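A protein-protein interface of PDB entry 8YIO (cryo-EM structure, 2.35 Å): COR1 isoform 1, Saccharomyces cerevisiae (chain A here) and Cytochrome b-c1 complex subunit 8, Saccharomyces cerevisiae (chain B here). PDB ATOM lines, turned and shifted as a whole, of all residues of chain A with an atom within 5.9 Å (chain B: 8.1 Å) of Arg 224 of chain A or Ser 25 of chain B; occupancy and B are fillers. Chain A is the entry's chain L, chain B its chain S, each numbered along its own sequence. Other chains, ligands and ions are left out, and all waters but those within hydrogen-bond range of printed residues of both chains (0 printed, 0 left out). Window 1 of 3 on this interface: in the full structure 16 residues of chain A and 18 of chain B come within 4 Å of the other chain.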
ATOM      1  N   GLU A 222      30.447   2.364  -4.294  1.00  0.00           N
ATOM      2  CA  GLU A 222      30.584   2.645  -5.718  1.00  0.00           C
ATOM      3  C   GLU A 222      29.429   3.522  -6.187  1.00  0.00           C
ATOM      4  O   GLU A 222      28.344   3.509  -5.604  1.00  0.00           O
ATOM      5  CB  GLU A 222      30.639   1.359  -6.548  1.00  0.00           C
ATOM      6  CG  GLU A 222      29.467   0.436  -6.339  1.00  0.00           C
ATOM      7  CD  GLU A 222      29.409  -0.671  -7.368  1.00  0.00           C
ATOM      8  OE1 GLU A 222      30.285  -0.702  -8.254  1.00  0.00           O
ATOM      9  OE2 GLU A 222      28.485  -1.507  -7.296  1.00  0.00           O
ATOM     10  N   VAL A 223      29.683   4.288  -7.246  1.00  0.00           N
ATOM     11  CA  VAL A 223      28.661   5.084  -7.919  1.00  0.00           C
ATOM     12  C   VAL A 223      28.900   5.003  -9.428  1.00  0.00           C
ATOM     13  O   VAL A 223      30.032   5.153  -9.895  1.00  0.00           O
ATOM     14  CB  VAL A 223      28.635   6.542  -7.395  1.00  0.00           C
ATOM     15  CG1 VAL A 223      30.018   7.204  -7.413  1.00  0.00           C
ATOM     16  CG2 VAL A 223      27.609   7.384  -8.141  1.00  0.00           C
ATOM     17  N   ARG A 224      27.842   4.713 -10.185  1.00  0.00           N
ATOM     18  CA  ARG A 224      27.920   4.520 -11.629  1.00  0.00           C
ATOM     19  C   ARG A 224      27.014   5.518 -12.336  1.00  0.00           C
ATOM     20  O   ARG A 224      25.824   5.605 -12.025  1.00  0.00           O
ATOM     21  CB  ARG A 224      27.519   3.094 -12.017  1.00  0.00           C
ATOM     22  CG  ARG A 224      28.479   2.028 -11.546  1.00  0.00           C
ATOM     23  CD  ARG A 224      27.915   0.636 -11.714  1.00  0.00           C
ATOM     24  NE  ARG A 224      28.669  -0.329 -10.923  1.00  0.00           N
ATOM     25  CZ  ARG A 224      29.418  -1.305 -11.426  1.00  0.00           C
ATOM     26  NH1 ARG A 224      30.070  -2.120 -10.611  1.00  0.00           N
ATOM     27  NH2 ARG A 224      29.514  -1.471 -12.735  1.00  0.00           N
ATOM     28  N   LEU A 225      27.570   6.261 -13.290  1.00  0.00           N
ATOM     29  CA  LEU A 225      26.814   7.243 -14.068  1.00  0.00           C
ATOM     30  C   LEU A 225      26.923   6.874 -15.547  1.00  0.00           C
ATOM     31  O   LEU A 225      27.703   7.461 -16.288  1.00  0.00           O
ATOM     32  CB  LEU A 225      27.334   8.675 -13.798  1.00  0.00           C
ATOM     33  CG  LEU A 225      27.352   9.199 -12.357  1.00  0.00           C
ATOM     34  CD1 LEU A 225      28.735   9.066 -11.738  1.00  0.00           C
ATOM     35  CD2 LEU A 225      26.876  10.633 -12.279  1.00  0.00           C
ATOM     36  N   ARG A 226      26.081   5.948 -15.991  1.00  0.00           N
ATOM     37  CA  ARG A 226      26.205   5.392 -17.333  1.00  0.00           C
ATOM     38  C   ARG A 226      25.629   6.345 -18.378  1.00  0.00           C
ATOM     39  O   ARG A 226      24.514   6.852 -18.225  1.00  0.00           O
ATOM     40  CB  ARG A 226      25.510   4.036 -17.403  1.00  0.00           C
ATOM     41  CG  ARG A 226      25.613   3.354 -18.746  1.00  0.00           C
ATOM     42  CD  ARG A 226      25.238   1.894 -18.657  1.00  0.00           C
ATOM     43  NE  ARG A 226      24.877   1.357 -19.961  1.00  0.00           N
ATOM     44  CZ  ARG A 226      24.577   0.084 -20.192  1.00  0.00           C
ATOM     45  NH1 ARG A 226      24.260  -0.310 -21.413  1.00  0.00           N
ATOM     46  NH2 ARG A 226      24.594  -0.791 -19.201  1.00  0.00           N
ATOM     47  N   ILE A 407      34.883   2.967  -6.047  1.00  0.00           N
ATOM     48  CA  ILE A 407      34.880   3.011  -7.509  1.00  0.00           C
ATOM     49  C   ILE A 407      33.931   4.111  -7.978  1.00  0.00           C
ATOM     50  O   ILE A 407      32.860   4.306  -7.398  1.00  0.00           O
ATOM     51  CB  ILE A 407      34.469   1.653  -8.133  1.00  0.00           C
ATOM     52  CG1 ILE A 407      35.088   0.464  -7.389  1.00  0.00           C
ATOM     53  CG2 ILE A 407      34.877   1.582  -9.592  1.00  0.00           C
ATOM     54  CD1 ILE A 407      34.449  -0.857  -7.700  1.00  0.00           C
ATOM     55  N   ALA A 408      34.331   4.836  -9.023  1.00  0.00           N
ATOM     56  CA  ALA A 408      33.457   5.776  -9.716  1.00  0.00           C
ATOM     57  C   ALA A 408      33.693   5.660 -11.216  1.00  0.00           C
ATOM     58  O   ALA A 408      34.796   5.334 -11.657  1.00  0.00           O
ATOM     59  CB  ALA A 408      33.679   7.218  -9.247  1.00  0.00           C
ATOM     60  N   GLY A 409      32.647   5.920 -11.998  1.00  0.00           N
ATOM     61  CA  GLY A 409      32.739   5.774 -13.441  1.00  0.00           C
ATOM     62  C   GLY A 409      31.635   6.426 -14.251  1.00  0.00           C
ATOM     63  O   GLY A 409      30.508   6.565 -13.769  1.00  0.00           O
ATOM     64  N   ILE A 413      30.236   2.172 -19.681  1.00  0.00           N
ATOM     65  CA  ILE A 413      30.803   1.380 -18.595  1.00  0.00           C
ATOM     66  C   ILE A 413      30.011   0.096 -18.382  1.00  0.00           C
ATOM     67  O   ILE A 413      29.939  -0.415 -17.261  1.00  0.00           O
ATOM     68  CB  ILE A 413      30.867   2.199 -17.294  1.00  0.00           C
ATOM     69  CG1 ILE A 413      29.529   2.899 -17.038  1.00  0.00           C
ATOM     70  CG2 ILE A 413      32.000   3.200 -17.356  1.00  0.00           C
ATOM     71  CD1 ILE A 413      29.372   3.440 -15.642  1.00  0.00           C
ATOM     72  N   LEU A 416      32.179  -2.894 -17.233  1.00  0.00           N
ATOM     73  CA  LEU A 416      32.704  -2.873 -15.875  1.00  0.00           C
ATOM     74  C   LEU A 416      31.877  -3.812 -15.006  1.00  0.00           C
ATOM     75  O   LEU A 416      30.667  -3.618 -14.851  1.00  0.00           O
ATOM     76  CB  LEU A 416      32.683  -1.452 -15.321  1.00  0.00           C
ATOM     77  CG  LEU A 416      33.205  -1.222 -13.902  1.00  0.00           C
ATOM     78  CD1 LEU A 416      34.705  -1.433 -13.835  1.00  0.00           C
ATOM     79  CD2 LEU A 416      32.841   0.170 -13.427  1.00  0.00           C
ATOM     80  N   LEU A 417      32.523  -4.830 -14.448  1.00  0.00           N
ATOM     81  CA  LEU A 417      31.833  -5.825 -13.646  1.00  0.00           C
ATOM     82  C   LEU A 417      31.481  -5.260 -12.272  1.00  0.00           C
ATOM     83  O   LEU A 417      31.901  -4.166 -11.890  1.00  0.00           O
ATOM     84  CB  LEU A 417      32.682  -7.085 -13.510  1.00  0.00           C
ATOM     85  CG  LEU A 417      32.954  -7.871 -14.795  1.00  0.00           C
ATOM     86  CD1 LEU A 417      33.635  -9.188 -14.485  1.00  0.00           C
ATOM     87  CD2 LEU A 417      31.678  -8.101 -15.588  1.00  0.00           C
ATOM     88  N   ASP A 418      30.706  -6.030 -11.516  1.00  0.00           N
ATOM     89  CA  ASP A 418      30.179  -5.538 -10.256  1.00  0.00           C
ATOM     90  C   ASP A 418      31.237  -5.606  -9.154  1.00  0.00           C
ATOM     91  O   ASP A 418      32.380  -6.016  -9.375  1.00  0.00           O
ATOM     92  CB  ASP A 418      28.934  -6.319  -9.861  1.00  0.00           C
ATOM     93  CG  ASP A 418      29.260  -7.679  -9.334  1.00  0.00           C
ATOM     94  OD1 ASP A 418      29.797  -8.514 -10.092  1.00  0.00           O
ATOM     95  OD2 ASP A 418      28.978  -7.902  -8.145  1.00  0.00           O
ATOM     96  N   TYR A 419      30.823  -5.228  -7.937  1.00  0.00           N
ATOM     97  CA  TYR A 419      31.759  -4.877  -6.870  1.00  0.00           C
ATOM     98  C   TYR A 419      32.555  -6.079  -6.364  1.00  0.00           C
ATOM     99  O   TYR A 419      33.766  -5.969  -6.150  1.00  0.00           O
ATOM    100  CB  TYR A 419      31.006  -4.215  -5.714  1.00  0.00           C
ATOM    101  CG  TYR A 419      31.904  -3.646  -4.637  1.00  0.00           C
ATOM    102  CD1 TYR A 419      32.456  -2.378  -4.766  1.00  0.00           C
ATOM    103  CD2 TYR A 419      32.202  -4.378  -3.490  1.00  0.00           C
ATOM    104  CE1 TYR A 419      33.280  -1.861  -3.791  1.00  0.00           C
ATOM    105  CE2 TYR A 419      33.030  -3.873  -2.521  1.00  0.00           C
ATOM    106  CZ  TYR A 419      33.561  -2.612  -2.670  1.00  0.00           C
ATOM    107  OH  TYR A 419      34.379  -2.104  -1.694  1.00  0.00           O
ATOM    108  N   ILE A 422      35.548  -7.312  -8.388  1.00  0.00           N
ATOM    109  CA  ILE A 422      36.703  -6.423  -8.316  1.00  0.00           C
ATOM    110  C   ILE A 422      37.325  -6.455  -6.924  1.00  0.00           C
ATOM    111  O   ILE A 422      38.548  -6.354  -6.777  1.00  0.00           O
ATOM    112  CB  ILE A 422      36.280  -5.002  -8.734  1.00  0.00           C
ATOM    113  CG1 ILE A 422      35.543  -5.052 -10.071  1.00  0.00           C
ATOM    114  CG2 ILE A 422      37.477  -4.073  -8.844  1.00  0.00           C
ATOM    115  CD1 ILE A 422      34.959  -3.734 -10.499  1.00  0.00           C
ATOM    116  N   GLY B  22      20.976   8.952 -18.019  1.00  0.00           N
ATOM    117  CA  GLY B  22      20.292   9.618 -16.932  1.00  0.00           C
ATOM    118  C   GLY B  22      20.068   8.802 -15.677  1.00  0.00           C
ATOM    119  O   GLY B  22      19.430   9.303 -14.748  1.00  0.00           O
ATOM    120  N   ILE B  23      20.576   7.575 -15.610  1.00  0.00           N
ATOM    121  CA  ILE B  23      20.351   6.677 -14.482  1.00  0.00           C
ATOM    122  C   ILE B  23      21.643   6.549 -13.687  1.00  0.00           C
ATOM    123  O   ILE B  23      22.697   6.233 -14.250  1.00  0.00           O
ATOM    124  CB  ILE B  23      19.855   5.300 -14.959  1.00  0.00           C
ATOM    125  CG1 ILE B  23      18.586   5.453 -15.798  1.00  0.00           C
ATOM    126  CG2 ILE B  23      19.617   4.370 -13.782  1.00  0.00           C
ATOM    127  CD1 ILE B  23      18.076   4.168 -16.382  1.00  0.00           C
ATOM    128  N   THR B  24      21.562   6.796 -12.382  1.00  0.00           N
ATOM    129  CA  THR B  24      22.679   6.646 -11.459  1.00  0.00           C
ATOM    130  C   THR B  24      22.384   5.515 -10.480  1.00  0.00           C
ATOM    131  O   THR B  24      21.246   5.355 -10.034  1.00  0.00           O
ATOM    132  CB  THR B  24      22.934   7.956 -10.699  1.00  0.00           C
ATOM    133  OG1 THR B  24      22.861   9.055 -11.612  1.00  0.00           O
ATOM    134  CG2 THR B  24      24.302   7.964 -10.044  1.00  0.00           C
ATOM    135  N   SER B  25      23.405   4.724 -10.148  1.00  0.00           N
ATOM    136  CA  SER B  25      23.263   3.633  -9.191  1.00  0.00           C
ATOM    137  C   SER B  25      24.299   3.747  -8.078  1.00  0.00           C
ATOM    138  O   SER B  25      25.394   4.276  -8.276  1.00  0.00           O
ATOM    139  CB  SER B  25      23.374   2.264  -9.877  1.00  0.00           C
ATOM    140  OG  SER B  25      24.526   2.181 -10.683  1.00  0.00           O
ATOM    141  N   TYR B  26      23.936   3.236  -6.900  1.00  0.00           N
ATOM    142  CA  TYR B  26      24.753   3.301  -5.694  1.00  0.00           C
ATOM    143  C   TYR B  26      24.767   1.940  -5.009  1.00  0.00           C
ATOM    144  O   TYR B  26      23.762   1.226  -5.024  1.00  0.00           O
ATOM    145  CB  TYR B  26      24.225   4.355  -4.706  1.00  0.00           C
ATOM    146  CG  TYR B  26      24.060   5.753  -5.263  1.00  0.00           C
ATOM    147  CD1 TYR B  26      22.864   6.152  -5.850  1.00  0.00           C
ATOM    148  CD2 TYR B  26      25.092   6.681  -5.181  1.00  0.00           C
ATOM    149  CE1 TYR B  26      22.705   7.426  -6.350  1.00  0.00           C
ATOM    150  CE2 TYR B  26      24.943   7.960  -5.675  1.00  0.00           C
ATOM    151  CZ  TYR B  26      23.746   8.327  -6.258  1.00  0.00           C
ATOM    152  OH  TYR B  26      23.587   9.595  -6.758  1.00  0.00           O
ATOM    153  N   ALA B  27      25.896   1.590  -4.394  1.00  0.00           N
ATOM    154  CA  ALA B  27      26.025   0.325  -3.680  1.00  0.00           C
ATOM    155  C   ALA B  27      27.069   0.459  -2.579  1.00  0.00           C
ATOM    156  O   ALA B  27      27.967   1.297  -2.649  1.00  0.00           O
ATOM    157  CB  ALA B  27      26.392  -0.822  -4.628  1.00  0.00           C
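The backbone carbonyl oxygen of Ala 27 of chain B is in hydrogen-bond range of the backbone NH of Glu 222 of chain A. The backbone carbonyl oxygen of Ser 25 of chain B is in hydrogen-bond range of the backbone NH of Arg 224 of chain A.
Of the 14 printed residues of chain A, 4 touch a printed residue of chain B. Printed residues of chain B that touch a printed residue of chain A: Ile 23, Thr 24, Ser 25, Tyr 26 and Ala 27. Hydrophobic or aromatic side chains of chain B that line the printed part of chain A: Tyr 26 and Ala 27. Among the printed residues, no Asp or Glu carboxylate lies within 4 Å of a Lys or Arg side-chain nitrogen of the other chain.
Arg 224 of chain A touches three residues of chain B. Gly 409 of chain A touches none of the printed residues of chain B. Printed residues of chain A within 4 Å of Thr 24 of chain B: Val 223 (3.9 Å) and Arg 224 (3.4 Å). Ser 25 of chain B touches two residues of chain A. Of the printed residues of chain A, Ala 27 of chain B touches Glu 222. The nearest residue of chain A that does not touch Ser 25 of chain B is Glu 222 of chain A (4.1 Å).
OE1 of Glu 222 of chain A is in salt-bridge range of NH1 of Arg 224 of chain A (2.8 Å). N of Val 223 of chain A is in hydrogen-bond range of O of Ile 407 of chain A, 3.2 Å away. The backbone carbonyl oxygen (O) of Val 223 of chain A is in hydrogen-bond range of the backbone NH (N) of Gly 409 of chain A (3.4 Å). NH2 of Arg 224 of chain A sits at hydrogen-bond distance from O of Leu 416 of chain A, at 3.2 Å. The guanidinium group (NH1) of Arg 224 of chain A is in hydrogen-bond range of the backbone carbonyl oxygen (O) of Leu 417 of chain A (3.0 Å).
Among the printed residues, merely in contact across the chains: Glu 222 of chain A with Tyr 26 of chain B (3.6 Å), Val 223 of chain A with Thr 24 of chain B (3.9 Å), Val 223 of chain A with Ser 25 of chain B (3.4 Å), Val 223 of chain A with Tyr 26 of chain B (3.7 Å), Arg 224 of chain A with Ile 23 of chain B (3.9 Å), Arg 224 of chain A with Thr 24 of chain B (3.4 Å) and Arg 226 of chain A with Ile 23 of chain B (3.8 Å).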
